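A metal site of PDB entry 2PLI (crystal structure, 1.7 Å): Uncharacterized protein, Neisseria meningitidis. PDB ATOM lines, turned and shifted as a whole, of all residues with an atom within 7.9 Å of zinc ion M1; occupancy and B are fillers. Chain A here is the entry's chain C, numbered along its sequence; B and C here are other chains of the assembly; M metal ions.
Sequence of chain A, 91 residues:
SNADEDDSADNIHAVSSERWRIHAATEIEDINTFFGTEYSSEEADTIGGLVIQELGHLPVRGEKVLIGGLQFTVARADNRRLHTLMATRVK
OE1 of Glu 27 of chain B is in salt-bridge range of NH2 of Arg 21 (2.9 Å). O of His 13 of chain A lies within hydrogen-bond range of N of Arg 21, at 2.7 Å. The backbone NH (N) of Asp 10 of chain C lies close to the side-chain hydroxyl (OG) of Ser 8 of chain C (3.1 Å). OD2 of Asp 10 of chain C sits at hydrogen-bond distance from ND1 of His 13 of chain C, 2.8 Å away.
Within 4 Å of zinc ion M1: Asp 10 of chain A, His 13 of chain A, Glu 27 of chain B and Asp 10 of chain C. Along chain A the residues within 4 Å of zinc ion M1 span positions 10 to 13. The nearest printed residue that does not touch zinc ion M1 is Ser 8 of chain C (4.3 Å).
Zinc ion M1 is bound by the side-chain carboxylate of Glu 27 of chain B (2.0 Å), the side-chain carboxylate of Asp 10 of chain A (2.0 Å), a ring nitrogen (ND1) of His 13 of chain A (2.0 Å) and the side-chain carboxylate of Asp 10 of chain C (2.1 Å). Slightly farther from zinc ion M1 lies OD2 of Asp 10 of chain C (2.7 Å).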
ATOM      1  N   ASP A  10       2.698 -21.799   3.206  1.00  0.00           N
ATOM      2  CA  ASP A  10       3.684 -22.906   3.312  1.00  0.00           C
ATOM      3  C   ASP A  10       5.026 -22.602   2.595  1.00  0.00           C
ATOM      4  O   ASP A  10       5.104 -22.422   1.357  1.00  0.00           O
ATOM      5  CB  ASP A  10       3.055 -24.194   2.774  1.00  0.00           C
ATOM      6  CG  ASP A  10       2.440 -24.006   1.430  1.00  0.00           C
ATOM      7  OD1 ASP A  10       1.979 -22.885   1.120  1.00  0.00           O
ATOM      8  OD2 ASP A  10       2.426 -24.951   0.695  1.00  0.00           O
ATOM      9  N   ASN A  11       6.086 -22.531   3.400  1.00  0.00           N
ATOM     10  CA  ASN A  11       7.434 -22.378   2.883  1.00  0.00           C
ATOM     11  C   ASN A  11       7.898 -23.647   2.202  1.00  0.00           C
ATOM     12  O   ASN A  11       8.863 -23.610   1.431  1.00  0.00           O
ATOM     13  CB  ASN A  11       8.394 -22.040   4.012  1.00  0.00           C
ATOM     14  CG  ASN A  11       8.315 -20.606   4.429  1.00  0.00           C
ATOM     15  OD1 ASN A  11       8.052 -19.708   3.620  1.00  0.00           O
ATOM     16  ND2 ASN A  11       8.585 -20.362   5.724  1.00  0.00           N
ATOM     17  N   ILE A  12       7.256 -24.769   2.509  1.00  0.00           N
ATOM     18  CA  ILE A  12       7.560 -26.052   1.900  1.00  0.00           C
ATOM     19  C   ILE A  12       6.225 -26.587   1.336  1.00  0.00           C
ATOM     20  O   ILE A  12       5.295 -26.945   2.081  1.00  0.00           O
ATOM     21  CB  ILE A  12       8.149 -27.090   2.900  1.00  0.00           C
ATOM     22  CG1 ILE A  12       9.397 -26.522   3.596  1.00  0.00           C
ATOM     23  CG2 ILE A  12       8.481 -28.392   2.151  1.00  0.00           C
ATOM     24  CD1 ILE A  12       9.925 -27.393   4.732  1.00  0.00           C
ATOM     25  N   HIS A  13       6.147 -26.543   0.019  1.00  0.00           N
ATOM     26  CA  HIS A  13       4.936 -26.883  -0.740  1.00  0.00           C
ATOM     27  C   HIS A  13       5.211 -28.119  -1.559  1.00  0.00           C
ATOM     28  O   HIS A  13       6.170 -28.148  -2.399  1.00  0.00           O
ATOM     29  CB  HIS A  13       4.631 -25.716  -1.687  1.00  0.00           C
ATOM     30  CG  HIS A  13       3.577 -26.010  -2.696  1.00  0.00           C
ATOM     31  ND1 HIS A  13       2.248 -25.693  -2.509  1.00  0.00           N
ATOM     32  CD2 HIS A  13       3.673 -26.560  -3.925  1.00  0.00           C
ATOM     33  CE1 HIS A  13       1.565 -26.066  -3.586  1.00  0.00           C
ATOM     34  NE2 HIS A  13       2.401 -26.624  -4.446  1.00  0.00           N
ATOM     35  N   ALA A  14       4.403 -29.152  -1.401  1.00  0.00           N
ATOM     36  CA  ALA A  14       4.527 -30.364  -2.268  1.00  0.00           C
ATOM     37  C   ALA A  14       3.925 -30.097  -3.637  1.00  0.00           C
ATOM     38  O   ALA A  14       2.715 -29.875  -3.765  1.00  0.00           O
ATOM     39  CB  ALA A  14       3.867 -31.584  -1.666  1.00  0.00           C
ATOM     40  N   VAL A  15       4.791 -30.075  -4.644  1.00  0.00           N
ATOM     41  CA  VAL A  15       4.376 -30.030  -6.034  1.00  0.00           C
ATOM     42  C   VAL A  15       3.749 -31.381  -6.438  1.00  0.00           C
ATOM     43  O   VAL A  15       2.694 -31.436  -7.094  1.00  0.00           O
ATOM     44  CB  VAL A  15       5.593 -29.650  -6.921  1.00  0.00           C
ATOM     45  CG1 VAL A  15       5.312 -29.875  -8.361  1.00  0.00           C
ATOM     46  CG2 VAL A  15       5.965 -28.143  -6.693  1.00  0.00           C
ATOM     47  N   ARG A  21       8.606 -27.663  -3.442  1.00  0.00           N
ATOM     48  CA  ARG A  21       9.022 -26.311  -3.768  1.00  0.00           C
ATOM     49  C   ARG A  21       9.266 -25.604  -2.444  1.00  0.00           C
ATOM     50  O   ARG A  21       8.356 -25.538  -1.593  1.00  0.00           O
ATOM     51  CB  ARG A  21       7.960 -25.566  -4.558  1.00  0.00           C
ATOM     52  CG  ARG A  21       8.207 -24.067  -4.689  1.00  0.00           C
ATOM     53  CD  ARG A  21       7.186 -23.462  -5.639  1.00  0.00           C
ATOM     54  NE  ARG A  21       5.875 -23.303  -5.047  1.00  0.00           N
ATOM     55  CZ  ARG A  21       4.727 -23.685  -5.599  1.00  0.00           C
ATOM     56  NH1 ARG A  21       4.665 -24.316  -6.754  1.00  0.00           N
ATOM     57  NH2 ARG A  21       3.587 -23.408  -4.977  1.00  0.00           N
ATOM     58  N   ASN B  11      -7.978 -23.905  -7.289  1.00  0.00           N
ATOM     59  CA  ASN B  11      -7.647 -22.534  -6.943  1.00  0.00           C
ATOM     60  C   ASN B  11      -7.754 -21.552  -8.091  1.00  0.00           C
ATOM     61  O   ASN B  11      -7.971 -20.367  -7.886  1.00  0.00           O
ATOM     62  CB  ASN B  11      -6.221 -22.465  -6.391  1.00  0.00           C
ATOM     63  CG  ASN B  11      -6.109 -22.974  -4.983  1.00  0.00           C
ATOM     64  OD1 ASN B  11      -5.115 -23.625  -4.644  1.00  0.00           O
ATOM     65  ND2 ASN B  11      -7.092 -22.676  -4.139  1.00  0.00           N
ATOM     66  N   ALA B  25      -5.570 -16.714  -2.263  1.00  0.00           N
ATOM     67  CA  ALA B  25      -4.499 -17.468  -1.554  1.00  0.00           C
ATOM     68  C   ALA B  25      -3.576 -18.304  -2.440  1.00  0.00           C
ATOM     69  O   ALA B  25      -2.616 -18.875  -1.951  1.00  0.00           O
ATOM     70  CB  ALA B  25      -5.088 -18.397  -0.459  1.00  0.00           C
ATOM     71  N   THR B  26      -3.882 -18.353  -3.727  1.00  0.00           N
ATOM     72  CA  THR B  26      -3.134 -19.169  -4.678  1.00  0.00           C
ATOM     73  C   THR B  26      -1.673 -18.699  -4.648  1.00  0.00           C
ATOM     74  O   THR B  26      -1.406 -17.476  -4.730  1.00  0.00           O
ATOM     75  CB  THR B  26      -3.681 -19.028  -6.109  1.00  0.00           C
ATOM     76  OG1 THR B  26      -5.069 -19.404  -6.119  1.00  0.00           O
ATOM     77  CG2 THR B  26      -2.908 -19.936  -7.076  1.00  0.00           C
ATOM     78  N   GLU B  27      -0.733 -19.638  -4.529  1.00  0.00           N
ATOM     79  CA  GLU B  27       0.694 -19.269  -4.469  1.00  0.00           C
ATOM     80  C   GLU B  27       1.196 -18.751  -5.800  1.00  0.00           C
ATOM     81  O   GLU B  27       0.816 -19.231  -6.853  1.00  0.00           O
ATOM     82  CB  GLU B  27       1.580 -20.428  -3.911  1.00  0.00           C
ATOM     83  CG  GLU B  27       1.165 -20.819  -2.475  1.00  0.00           C
ATOM     84  CD  GLU B  27       1.604 -22.232  -2.060  1.00  0.00           C
ATOM     85  OE1 GLU B  27       2.810 -22.460  -2.298  1.00  0.00           O
ATOM     86  OE2 GLU B  27       0.843 -23.083  -1.449  1.00  0.00           O
ATOM     87  N   GLU B  29       3.949 -18.992  -7.370  1.00  0.00           N
ATOM     88  CA  GLU B  29       4.598 -19.928  -8.253  1.00  0.00           C
ATOM     89  C   GLU B  29       3.575 -20.736  -9.040  1.00  0.00           C
ATOM     90  O   GLU B  29       3.854 -21.136 -10.173  1.00  0.00           O
ATOM     91  CB  GLU B  29       5.543 -20.844  -7.518  1.00  0.00           C
ATOM     92  CG  GLU B  29       6.554 -20.060  -6.655  1.00  0.00           C
ATOM     93  CD  GLU B  29       6.159 -19.855  -5.206  1.00  0.00           C
ATOM     94  OE1 GLU B  29       4.983 -19.678  -4.880  1.00  0.00           O
ATOM     95  OE2 GLU B  29       7.082 -19.890  -4.293  1.00  0.00           O
ATOM     96  N   ASP B  30       2.432 -21.016  -8.429  1.00  0.00           N
ATOM     97  CA  ASP B  30       1.379 -21.761  -9.134  1.00  0.00           C
ATOM     98  C   ASP B  30       0.694 -20.924 -10.235  1.00  0.00           C
ATOM     99  O   ASP B  30       0.298 -21.462 -11.277  1.00  0.00           O
ATOM    100  CB  ASP B  30       0.413 -22.386  -8.135  1.00  0.00           C
ATOM    101  CG  ASP B  30       1.114 -23.478  -7.325  1.00  0.00           C
ATOM    102  OD1 ASP B  30       1.915 -24.276  -7.906  1.00  0.00           O
ATOM    103  OD2 ASP B  30       0.915 -23.489  -6.121  1.00  0.00           O
ATOM    104  N   SER C   8      -3.457 -23.774   4.452  1.00  0.00           N
ATOM    105  CA  SER C   8      -2.865 -23.324   3.148  1.00  0.00           C
ATOM    106  C   SER C   8      -3.921 -23.477   2.062  1.00  0.00           C
ATOM    107  O   SER C   8      -5.014 -23.937   2.336  1.00  0.00           O
ATOM    108  CB  SER C   8      -1.587 -24.115   2.815  1.00  0.00           C
ATOM    109  OG  SER C   8      -1.842 -25.241   1.984  1.00  0.00           O
ATOM    110  N   ALA C   9      -3.581 -23.124   0.821  1.00  0.00           N
ATOM    111  CA  ALA C   9      -4.558 -23.224  -0.269  1.00  0.00           C
ATOM    112  C   ALA C   9      -4.407 -24.543  -1.057  1.00  0.00           C
ATOM    113  O   ALA C   9      -5.125 -24.765  -2.016  1.00  0.00           O
ATOM    114  CB  ALA C   9      -4.449 -22.057  -1.187  1.00  0.00           C
ATOM    115  N   ASP C  10      -3.510 -25.410  -0.623  1.00  0.00           N
ATOM    116  CA  ASP C  10      -3.225 -26.665  -1.297  1.00  0.00           C
ATOM    117  C   ASP C  10      -4.429 -27.608  -1.175  1.00  0.00           C
ATOM    118  O   ASP C  10      -4.835 -27.919  -0.039  1.00  0.00           O
ATOM    119  CB  ASP C  10      -2.048 -27.401  -0.597  1.00  0.00           C
ATOM    120  CG  ASP C  10      -0.745 -26.622  -0.543  1.00  0.00           C
ATOM    121  OD1 ASP C  10      -0.651 -25.518  -1.093  1.00  0.00           O
ATOM    122  OD2 ASP C  10       0.212 -27.116   0.105  1.00  0.00           O
ATOM    123  N   ASN C  11      -4.963 -28.141  -2.281  1.00  0.00           N
ATOM    124  CA  ASN C  11      -5.989 -29.174  -2.101  1.00  0.00           C
ATOM    125  C   ASN C  11      -5.346 -30.466  -1.577  1.00  0.00           C
ATOM    126  O   ASN C  11      -6.010 -31.245  -0.953  1.00  0.00           O
ATOM    127  CB  ASN C  11      -6.833 -29.452  -3.339  1.00  0.00           C
ATOM    128  CG  ASN C  11      -6.053 -29.663  -4.584  1.00  0.00           C
ATOM    129  OD1 ASN C  11      -4.863 -30.012  -4.575  1.00  0.00           O
ATOM    130  ND2 ASN C  11      -6.748 -29.423  -5.740  1.00  0.00           N
ATOM    131  N   ILE C  12      -4.070 -30.662  -1.885  1.00  0.00           N
ATOM    132  CA  ILE C  12      -3.286 -31.784  -1.369  1.00  0.00           C
ATOM    133  C   ILE C  12      -2.114 -31.184  -0.624  1.00  0.00           C
ATOM    134  O   ILE C  12      -1.163 -30.725  -1.266  1.00  0.00           O
ATOM    135  CB  ILE C  12      -2.751 -32.718  -2.491  1.00  0.00           C
ATOM    136  CG1 ILE C  12      -3.874 -33.239  -3.395  1.00  0.00           C
ATOM    137  CG2 ILE C  12      -1.973 -33.899  -1.892  1.00  0.00           C
ATOM    138  CD1 ILE C  12      -3.405 -34.057  -4.585  1.00  0.00           C
ATOM    139  N   HIS C  13      -2.191 -31.159   0.698  1.00  0.00           N
ATOM    140  CA  HIS C  13      -1.268 -30.378   1.516  1.00  0.00           C
ATOM    141  C   HIS C  13      -0.362 -31.281   2.281  1.00  0.00           C
ATOM    142  O   HIS C  13      -0.831 -32.080   3.071  1.00  0.00           O
ATOM    143  CB  HIS C  13      -2.045 -29.554   2.497  1.00  0.00           C
ATOM    144  CG  HIS C  13      -1.183 -28.687   3.333  1.00  0.00           C
ATOM    145  ND1 HIS C  13      -0.318 -27.769   2.785  1.00  0.00           N
ATOM    146  CD2 HIS C  13      -1.059 -28.601   4.674  1.00  0.00           C
ATOM    147  CE1 HIS C  13       0.345 -27.172   3.772  1.00  0.00           C
ATOM    148  NE2 HIS C  13      -0.089 -27.671   4.912  1.00  0.00           N
ATOM    149  N   ALA C  14       0.931 -31.186   2.072  1.00  0.00           N
ATOM    150  CA  ALA C  14       1.842 -32.027   2.826  1.00  0.00           C
ATOM    151  C   ALA C  14       1.988 -31.438   4.228  1.00  0.00           C
ATOM    152  O   ALA C  14       2.575 -30.368   4.370  1.00  0.00           O
ATOM    153  CB  ALA C  14       3.203 -32.103   2.146  1.00  0.00           C
HETATM  154 ZN    ZN M   1       1.316 -24.910  -0.921  1.00  0.00          ZN
HETATM  155 ZN    ZN M   2       5.906 -19.787  -2.691  1.00  0.00          ZN
